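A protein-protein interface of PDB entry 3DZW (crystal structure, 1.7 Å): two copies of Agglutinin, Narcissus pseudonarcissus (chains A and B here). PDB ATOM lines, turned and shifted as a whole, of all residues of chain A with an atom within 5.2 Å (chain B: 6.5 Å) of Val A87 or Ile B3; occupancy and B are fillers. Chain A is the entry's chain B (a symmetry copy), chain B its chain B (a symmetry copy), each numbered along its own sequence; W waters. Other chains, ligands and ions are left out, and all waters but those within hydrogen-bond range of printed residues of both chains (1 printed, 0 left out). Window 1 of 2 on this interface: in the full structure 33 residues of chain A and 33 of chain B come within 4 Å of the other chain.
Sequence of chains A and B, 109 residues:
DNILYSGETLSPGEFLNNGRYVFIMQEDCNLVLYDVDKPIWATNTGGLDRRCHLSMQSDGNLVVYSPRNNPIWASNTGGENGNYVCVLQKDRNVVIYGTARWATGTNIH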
ATOM      1  N   ASN A   2       7.650  -8.688 -12.897  1.00  0.00           N
ATOM      2  CA  ASN A   2       8.854  -9.030 -13.677  1.00  0.00           C
ATOM      3  C   ASN A   2       9.126  -8.044 -14.843  1.00  0.00           C
ATOM      4  O   ASN A   2      10.110  -8.197 -15.554  1.00  0.00           O
ATOM      5  CB  ASN A   2       8.812 -10.498 -14.201  1.00  0.00           C
ATOM      6  CG  ASN A   2       7.625 -10.780 -15.153  1.00  0.00           C
ATOM      7  OD1 ASN A   2       6.629 -10.058 -15.164  1.00  0.00           O
ATOM      8  ND2 ASN A   2       7.743 -11.888 -15.953  1.00  0.00           N
ATOM      9  N   ILE A   3       8.261  -7.014 -15.003  1.00  0.00           N
ATOM     10  CA  ILE A   3       8.408  -6.048 -16.088  1.00  0.00           C
ATOM     11  C   ILE A   3       8.313  -4.593 -15.647  1.00  0.00           C
ATOM     12  O   ILE A   3       7.476  -4.239 -14.786  1.00  0.00           O
ATOM     13  CB  ILE A   3       7.296  -6.254 -17.183  1.00  0.00           C
ATOM     14  CG1 ILE A   3       7.327  -7.668 -17.740  1.00  0.00           C
ATOM     15  CG2 ILE A   3       7.444  -5.240 -18.325  1.00  0.00           C
ATOM     16  CD1 ILE A   3       6.212  -7.943 -18.771  1.00  0.00           C
ATOM     17  N   LEU A   4       9.187  -3.753 -16.226  1.00  0.00           N
ATOM     18  CA  LEU A   4       9.161  -2.328 -16.018  1.00  0.00           C
ATOM     19  C   LEU A   4       8.787  -1.766 -17.398  1.00  0.00           C
ATOM     20  O   LEU A   4       9.585  -1.826 -18.342  1.00  0.00           O
ATOM     21  CB  LEU A   4      10.498  -1.773 -15.534  1.00  0.00           C
ATOM     22  CG  LEU A   4      10.526  -0.260 -15.238  1.00  0.00           C
ATOM     23  CD1 LEU A   4       9.568   0.103 -14.094  1.00  0.00           C
ATOM     24  CD2 LEU A   4      11.932   0.217 -14.913  1.00  0.00           C
ATOM     25  N   LEU A  16      12.263  -5.381  -9.361  1.00  0.00           N
ATOM     26  CA  LEU A  16      11.589  -6.362 -10.179  1.00  0.00           C
ATOM     27  C   LEU A  16      12.005  -7.689  -9.591  1.00  0.00           C
ATOM     28  O   LEU A  16      13.112  -7.804  -9.039  1.00  0.00           O
ATOM     29  CB  LEU A  16      12.008  -6.299 -11.650  1.00  0.00           C
ATOM     30  CG  LEU A  16      11.777  -5.009 -12.442  1.00  0.00           C
ATOM     31  CD1 LEU A  16      12.281  -5.171 -13.877  1.00  0.00           C
ATOM     32  CD2 LEU A  16      10.310  -4.615 -12.429  1.00  0.00           C
ATOM     33  N   VAL A  85       9.626  -2.457 -23.166  1.00  0.00           N
ATOM     34  CA  VAL A  85       9.592  -3.193 -21.899  1.00  0.00           C
ATOM     35  C   VAL A  85      10.987  -3.639 -21.458  1.00  0.00           C
ATOM     36  O   VAL A  85      11.794  -4.045 -22.281  1.00  0.00           O
ATOM     37  CB  VAL A  85       8.668  -4.478 -21.946  1.00  0.00           C
ATOM     38  CG1 VAL A  85       7.198  -4.098 -22.076  1.00  0.00           C
ATOM     39  CG2 VAL A  85       9.107  -5.461 -23.067  1.00  0.00           C
ATOM     40  N   CYS A  86      11.258  -3.513 -20.143  1.00  0.00           N
ATOM     41  CA  CYS A  86      12.498  -3.992 -19.517  1.00  0.00           C
ATOM     42  C   CYS A  86      12.039  -5.190 -18.709  1.00  0.00           C
ATOM     43  O   CYS A  86      11.264  -5.031 -17.756  1.00  0.00           O
ATOM     44  CB  CYS A  86      13.127  -2.964 -18.628  1.00  0.00           C
ATOM     45  SG  CYS A  86      14.615  -3.570 -17.707  1.00  0.00           S
ATOM     46  N   VAL A  87      12.511  -6.385 -19.077  1.00  0.00           N
ATOM     47  CA  VAL A  87      12.072  -7.623 -18.440  1.00  0.00           C
ATOM     48  C   VAL A  87      13.115  -8.442 -17.689  1.00  0.00           C
ATOM     49  O   VAL A  87      14.199  -8.722 -18.226  1.00  0.00           O
ATOM     50  CB  VAL A  87      11.483  -8.597 -19.545  1.00  0.00           C
ATOM     51  CG1 VAL A  87      10.920  -9.894 -18.921  1.00  0.00           C
ATOM     52  CG2 VAL A  87      10.419  -7.896 -20.384  1.00  0.00           C
ATOM     53  N   LEU A  88      12.797  -8.808 -16.438  1.00  0.00           N
ATOM     54  CA  LEU A  88      13.653  -9.659 -15.645  1.00  0.00           C
ATOM     55  C   LEU A  88      13.122 -11.039 -15.970  1.00  0.00           C
ATOM     56  O   LEU A  88      12.075 -11.450 -15.465  1.00  0.00           O
ATOM     57  CB  LEU A  88      13.554  -9.338 -14.157  1.00  0.00           C
ATOM     58  CG  LEU A  88      14.560 -10.027 -13.206  1.00  0.00           C
ATOM     59  CD1 LEU A  88      14.322  -9.573 -11.767  1.00  0.00           C
ATOM     60  CD2 LEU A  88      14.498 -11.539 -13.292  1.00  0.00           C
ATOM     61  N   GLN A  89      13.836 -11.743 -16.849  1.00  0.00           N
ATOM     62  CA  GLN A  89      13.406 -13.069 -17.346  1.00  0.00           C
ATOM     63  C   GLN A  89      13.636 -14.294 -16.434  1.00  0.00           C
ATOM     64  O   GLN A  89      14.446 -14.273 -15.524  1.00  0.00           O
ATOM     65  CB  GLN A  89      14.082 -13.315 -18.722  1.00  0.00           C
ATOM     66  CG  GLN A  89      13.792 -12.177 -19.750  1.00  0.00           C
ATOM     67  CD  GLN A  89      14.363 -12.434 -21.141  1.00  0.00           C
ATOM     68  OE1 GLN A  89      14.004 -11.739 -22.094  1.00  0.00           O
ATOM     69  NE2 GLN A  89      15.235 -13.443 -21.269  1.00  0.00           N
ATOM     70  N   ASN A  93      18.261 -13.410 -17.397  1.00  0.00           N
ATOM     71  CA  ASN A  93      18.738 -12.308 -18.198  1.00  0.00           C
ATOM     72  C   ASN A  93      17.782 -11.134 -17.990  1.00  0.00           C
ATOM     73  O   ASN A  93      16.593 -11.348 -17.719  1.00  0.00           O
ATOM     74  CB  ASN A  93      18.811 -12.717 -19.677  1.00  0.00           C
ATOM     75  CG  ASN A  93      19.853 -11.882 -20.504  1.00  0.00           C
ATOM     76  OD1 ASN A  93      20.542 -11.000 -19.974  1.00  0.00           O
ATOM     77  ND2 ASN A  93      19.966 -12.202 -21.801  1.00  0.00           N
ATOM     78  N   VAL A  94      18.312  -9.900 -18.064  1.00  0.00           N
ATOM     79  CA  VAL A  94      17.507  -8.667 -17.968  1.00  0.00           C
ATOM     80  C   VAL A  94      17.603  -8.078 -19.383  1.00  0.00           C
ATOM     81  O   VAL A  94      18.713  -7.781 -19.860  1.00  0.00           O
ATOM     82  CB  VAL A  94      18.008  -7.707 -16.909  1.00  0.00           C
ATOM     83  CG1 VAL A  94      17.168  -6.418 -16.905  1.00  0.00           C
ATOM     84  CG2 VAL A  94      17.975  -8.369 -15.530  1.00  0.00           C
ATOM     85  N   VAL A  95      16.452  -7.923 -20.055  1.00  0.00           N
ATOM     86  CA  VAL A  95      16.436  -7.493 -21.459  1.00  0.00           C
ATOM     87  C   VAL A  95      15.410  -6.434 -21.830  1.00  0.00           C
ATOM     88  O   VAL A  95      14.277  -6.462 -21.344  1.00  0.00           O
ATOM     89  CB  VAL A  95      16.147  -8.746 -22.372  1.00  0.00           C
ATOM     90  CG1 VAL A  95      16.222  -8.381 -23.852  1.00  0.00           C
ATOM     91  CG2 VAL A  95      17.099  -9.879 -22.055  1.00  0.00           C
ATOM     92  N   ILE A  96      15.819  -5.502 -22.726  1.00  0.00           N
ATOM     93  CA  ILE A  96      14.938  -4.444 -23.239  1.00  0.00           C
ATOM     94  C   ILE A  96      14.415  -4.834 -24.627  1.00  0.00           C
ATOM     95  O   ILE A  96      15.217  -5.109 -25.533  1.00  0.00           O
ATOM     96  CB  ILE A  96      15.652  -3.089 -23.363  1.00  0.00           C
ATOM     97  CG1 ILE A  96      16.109  -2.582 -22.003  1.00  0.00           C
ATOM     98  CG2 ILE A  96      14.719  -2.049 -23.995  1.00  0.00           C
ATOM     99  CD1 ILE A  96      16.930  -1.271 -22.072  1.00  0.00           C
ATOM    100  N   TYR A  97      13.077  -4.868 -24.791  1.00  0.00           N
ATOM    101  CA  TYR A  97      12.434  -5.200 -26.078  1.00  0.00           C
ATOM    102  C   TYR A  97      11.576  -4.050 -26.573  1.00  0.00           C
ATOM    103  O   TYR A  97      10.945  -3.366 -25.786  1.00  0.00           O
ATOM    104  CB  TYR A  97      11.514  -6.425 -25.962  1.00  0.00           C
ATOM    105  CG  TYR A  97      12.162  -7.765 -25.598  1.00  0.00           C
ATOM    106  CD1 TYR A  97      12.241  -8.187 -24.273  1.00  0.00           C
ATOM    107  CD2 TYR A  97      12.636  -8.631 -26.594  1.00  0.00           C
ATOM    108  CE1 TYR A  97      12.807  -9.428 -23.937  1.00  0.00           C
ATOM    109  CE2 TYR A  97      13.198  -9.859 -26.274  1.00  0.00           C
ATOM    110  CZ  TYR A  97      13.283 -10.257 -24.940  1.00  0.00           C
ATOM    111  OH  TYR A  97      13.839 -11.490 -24.627  1.00  0.00           O
ATOM    112  N   ASP B   1       2.531 -17.977 -15.934  1.00  0.00           N
ATOM    113  CA  ASP B   1       3.452 -17.199 -16.789  1.00  0.00           C
ATOM    114  C   ASP B   1       2.712 -16.125 -17.549  1.00  0.00           C
ATOM    115  O   ASP B   1       1.625 -16.378 -18.078  1.00  0.00           O
ATOM    116  CB  ASP B   1       4.143 -18.115 -17.803  1.00  0.00           C
ATOM    117  CG  ASP B   1       5.013 -19.168 -17.153  1.00  0.00           C
ATOM    118  OD1 ASP B   1       5.799 -19.807 -17.884  1.00  0.00           O
ATOM    119  OD2 ASP B   1       4.922 -19.352 -15.920  1.00  0.00           O
ATOM    120  N   ASN B   2       3.294 -14.922 -17.620  1.00  0.00           N
ATOM    121  CA  ASN B   2       2.678 -13.821 -18.384  1.00  0.00           C
ATOM    122  C   ASN B   2       3.371 -13.565 -19.748  1.00  0.00           C
ATOM    123  O   ASN B   2       2.943 -12.696 -20.496  1.00  0.00           O
ATOM    124  CB  ASN B   2       2.604 -12.504 -17.553  1.00  0.00           C
ATOM    125  CG  ASN B   2       3.989 -11.967 -17.122  1.00  0.00           C
ATOM    126  OD1 ASN B   2       4.978 -12.699 -17.091  1.00  0.00           O
ATOM    127  ND2 ASN B   2       4.037 -10.646 -16.756  1.00  0.00           N
ATOM    128  N   ILE B   3       4.421 -14.357 -20.073  1.00  0.00           N
ATOM    129  CA  ILE B   3       5.163 -14.179 -21.318  1.00  0.00           C
ATOM    130  C   ILE B   3       5.388 -15.466 -22.101  1.00  0.00           C
ATOM    131  O   ILE B   3       5.672 -16.533 -21.511  1.00  0.00           O
ATOM    132  CB  ILE B   3       6.588 -13.569 -21.045  1.00  0.00           C
ATOM    133  CG1 ILE B   3       6.488 -12.244 -20.307  1.00  0.00           C
ATOM    134  CG2 ILE B   3       7.373 -13.381 -22.351  1.00  0.00           C
ATOM    135  CD1 ILE B   3       7.862 -11.636 -19.955  1.00  0.00           C
ATOM    136  N   LEU B   4       5.243 -15.367 -23.433  1.00  0.00           N
ATOM    137  CA  LEU B   4       5.534 -16.451 -24.337  1.00  0.00           C
ATOM    138  C   LEU B   4       6.740 -15.941 -25.140  1.00  0.00           C
ATOM    139  O   LEU B   4       6.611 -15.017 -25.954  1.00  0.00           O
ATOM    140  CB  LEU B   4       4.360 -16.794 -25.251  1.00  0.00           C
ATOM    141  CG  LEU B   4       4.584 -17.984 -26.206  1.00  0.00           C
ATOM    142  CD1 LEU B   4       4.810 -19.290 -25.431  1.00  0.00           C
ATOM    143  CD2 LEU B   4       3.423 -18.145 -27.175  1.00  0.00           C
ATOM    144  N   TYR B   5       7.920 -16.509 -24.866  1.00  0.00           N
ATOM    145  CA  TYR B   5       9.166 -16.093 -25.539  1.00  0.00           C
ATOM    146  C   TYR B   5       9.292 -16.672 -26.931  1.00  0.00           C
ATOM    147  O   TYR B   5       8.723 -17.726 -27.223  1.00  0.00           O
ATOM    148  CB  TYR B   5      10.385 -16.510 -24.696  1.00  0.00           C
ATOM    149  CG  TYR B   5      10.475 -15.826 -23.341  1.00  0.00           C
ATOM    150  CD1 TYR B   5       9.847 -16.365 -22.213  1.00  0.00           C
ATOM    151  CD2 TYR B   5      11.186 -14.634 -23.192  1.00  0.00           C
ATOM    152  CE1 TYR B   5       9.931 -15.735 -20.974  1.00  0.00           C
ATOM    153  CE2 TYR B   5      11.274 -13.996 -21.967  1.00  0.00           C
ATOM    154  CZ  TYR B   5      10.649 -14.543 -20.858  1.00  0.00           C
ATOM    155  OH  TYR B   5      10.743 -13.900 -19.637  1.00  0.00           O
ATOM    156  N   GLU B   8       9.246 -20.564 -28.272  1.00  0.00           N
ATOM    157  CA  GLU B   8       8.333 -21.364 -27.433  1.00  0.00           C
ATOM    158  C   GLU B   8       6.960 -21.489 -28.063  1.00  0.00           C
ATOM    159  O   GLU B   8       6.602 -20.719 -28.976  1.00  0.00           O
ATOM    160  CB  GLU B   8       8.180 -20.739 -26.039  1.00  0.00           C
ATOM    161  CG  GLU B   8       9.477 -20.644 -25.231  1.00  0.00           C
ATOM    162  CD  GLU B   8       9.264 -20.078 -23.789  1.00  0.00           C
ATOM    163  OE1 GLU B   8       8.285 -19.290 -23.554  1.00  0.00           O
ATOM    164  OE2 GLU B   8      10.084 -20.412 -22.905  1.00  0.00           O
ATOM    165  N   LEU B  16      -1.403 -18.338 -20.934  1.00  0.00           N
ATOM    166  CA  LEU B  16      -0.686 -17.301 -20.231  1.00  0.00           C
ATOM    167  C   LEU B  16      -1.697 -16.740 -19.258  1.00  0.00           C
ATOM    168  O   LEU B  16      -2.905 -16.757 -19.541  1.00  0.00           O
ATOM    169  CB  LEU B  16      -0.191 -16.187 -21.156  1.00  0.00           C
ATOM    170  CG  LEU B  16       0.775 -16.529 -22.293  1.00  0.00           C
ATOM    171  CD1 LEU B  16       1.123 -15.271 -23.091  1.00  0.00           C
ATOM    172  CD2 LEU B  16       2.035 -17.191 -21.760  1.00  0.00           C
ATOM    173  N   ASN B  17      -1.244 -16.289 -18.093  1.00  0.00           N
ATOM    174  CA  ASN B  17      -2.163 -15.695 -17.098  1.00  0.00           C
ATOM    175  C   ASN B  17      -1.567 -14.487 -16.400  1.00  0.00           C
ATOM    176  O   ASN B  17      -0.337 -14.380 -16.247  1.00  0.00           O
ATOM    177  CB  ASN B  17      -2.631 -16.730 -16.030  1.00  0.00           C
ATOM    178  CG  ASN B  17      -1.483 -17.226 -15.122  1.00  0.00           C
ATOM    179  OD1 ASN B  17      -0.648 -18.051 -15.530  1.00  0.00           O
ATOM    180  ND2 ASN B  17      -1.494 -16.777 -13.858  1.00  0.00           N
ATOM    181  N   TYR B  84      12.112 -12.068 -29.526  1.00  0.00           N
ATOM    182  CA  TYR B  84      10.844 -11.369 -29.306  1.00  0.00           C
ATOM    183  C   TYR B  84      10.084 -11.924 -28.107  1.00  0.00           C
ATOM    184  O   TYR B  84      10.410 -13.006 -27.594  1.00  0.00           O
ATOM    185  CB  TYR B  84       9.946 -11.510 -30.539  1.00  0.00           C
ATOM    186  CG  TYR B  84      10.516 -10.954 -31.841  1.00  0.00           C
ATOM    187  CD1 TYR B  84      11.396 -11.705 -32.622  1.00  0.00           C
ATOM    188  CD2 TYR B  84      10.134  -9.705 -32.310  1.00  0.00           C
ATOM    189  CE1 TYR B  84      11.905 -11.200 -33.822  1.00  0.00           C
ATOM    190  CE2 TYR B  84      10.639  -9.196 -33.505  1.00  0.00           C
ATOM    191  CZ  TYR B  84      11.518  -9.946 -34.251  1.00  0.00           C
ATOM    192  OH  TYR B  84      12.008  -9.432 -35.442  1.00  0.00           O
ATOM    193  N   VAL B  85       9.061 -11.178 -27.664  1.00  0.00           N
ATOM    194  CA  VAL B  85       8.193 -11.604 -26.563  1.00  0.00           C
ATOM    195  C   VAL B  85       6.727 -11.249 -26.819  1.00  0.00           C
ATOM    196  O   VAL B  85       6.432 -10.183 -27.339  1.00  0.00           O
ATOM    197  CB  VAL B  85       8.602 -10.982 -25.165  1.00  0.00           C
ATOM    198  CG1 VAL B  85       9.939 -11.536 -24.684  1.00  0.00           C
ATOM    199  CG2 VAL B  85       8.607  -9.429 -25.206  1.00  0.00           C
ATOM    200  N   CYS B  86       5.824 -12.190 -26.476  1.00  0.00           N
ATOM    201  CA  CYS B  86       4.371 -11.986 -26.541  1.00  0.00           C
ATOM    202  C   CYS B  86       3.966 -11.901 -25.082  1.00  0.00           C
ATOM    203  O   CYS B  86       4.097 -12.889 -24.347  1.00  0.00           O
ATOM    204  CB  CYS B  86       3.662 -13.117 -27.222  1.00  0.00           C
ATOM    205  SG  CYS B  86       1.816 -12.971 -27.203  1.00  0.00           S
ATOM    206  N   VAL B  87       3.472 -10.734 -24.658  1.00  0.00           N
ATOM    207  CA  VAL B  87       3.134 -10.496 -23.258  1.00  0.00           C
ATOM    208  C   VAL B  87       1.676 -10.212 -22.919  1.00  0.00           C
ATOM    209  O   VAL B  87       1.038  -9.356 -23.554  1.00  0.00           O
ATOM    210  CB  VAL B  87       3.944  -9.238 -22.733  1.00  0.00           C
ATOM    211  CG1 VAL B  87       3.697  -8.985 -21.228  1.00  0.00           C
ATOM    212  CG2 VAL B  87       5.436  -9.387 -23.016  1.00  0.00           C
ATOM    213  N   LEU B  88       1.141 -10.946 -21.932  1.00  0.00           N
ATOM    214  CA  LEU B  88      -0.202 -10.722 -21.449  1.00  0.00           C
ATOM    215  C   LEU B  88       0.024  -9.735 -20.322  1.00  0.00           C
ATOM    216  O   LEU B  88       0.463 -10.107 -19.232  1.00  0.00           O
ATOM    217  CB  LEU B  88      -0.855 -12.012 -20.963  1.00  0.00           C
ATOM    218  CG  LEU B  88      -2.359 -11.964 -20.607  1.00  0.00           C
ATOM    219  CD1 LEU B  88      -2.839 -13.344 -20.161  1.00  0.00           C
ATOM    220  CD2 LEU B  88      -2.671 -10.934 -19.540  1.00  0.00           C
HETATM  221  O   HOH W   1      12.995 -13.626 -26.467  1.00  0.00           O
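Water W1 bridges the backbone carbonyl oxygen of Tyr B84 (2.9 Å) and the side-chain hydroxyl of Tyr A97 (2.9 Å).
The side-chain amide oxygen (OD1) of Asn B2 is in hydrogen-bond range of the side-chain amide nitrogen (ND2) of Asn A2 (3.1 Å).
Of the printed residues of chain B, Val A87 touches Ile B3 (3.7 Å). Of the printed residues of chain A, Ile B3 touches Val A87 (3.7 Å). Printed residues of chain B within 4 Å of Tyr A97: Val B85. Printed residues of chain A within 4 Å of Val B87: Ile A3. The nearest residue of chain B that does not touch Val A87 is Tyr B5 (4.1 Å).
Asn B2 touches its own counterpart, Asn A2. Ile A3 touches Val B87, and with the chains exchanged Val A87 touches Ile B3. Of the 5 pairs that touch across the chains among the printed residues, 3 have their exchanged pair printed and touching as well.
Among the printed residues, merely in contact across the chains: Gln A89 with Tyr B5, Tyr A97 with Val B85, Ile A3 with Val B87 and Val A87 with Ile B3.
The backbone NH (N) of Val A87 is in hydrogen-bond range of the backbone carbonyl oxygen (O) of Val A95, at 2.9 Å. The backbone carbonyl oxygen of Asn A2 is in hydrogen-bond range of the backbone NH of Leu A88, at 2.9 Å. OE1 of Gln A89 sits at hydrogen-bond distance from OH of Tyr A97, at 2.6 Å. The backbone carbonyl oxygen (O) of Val A85 lies within hydrogen-bond range of the backbone NH (N) of Tyr A97 (2.9 Å). The backbone NH of Leu B88 sits at hydrogen-bond distance from the backbone carbonyl oxygen of Asn B2 (2.9 Å). OE1 of Glu B8 is in hydrogen-bond range of N of Tyr B5 (3.1 Å).
Of the 13 printed residues of chain B, 5 touch a printed residue of chain A. Hydrophobic or aromatic side chains of chain B within 4 Å of the printed part of chain A: Ile B3, Tyr B5, Val B85 and Val B87. Along chain B the printed residues that touch a printed residue of chain A span positions 2 to 87. Among the printed residues, 5 pairs touch across the chains.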
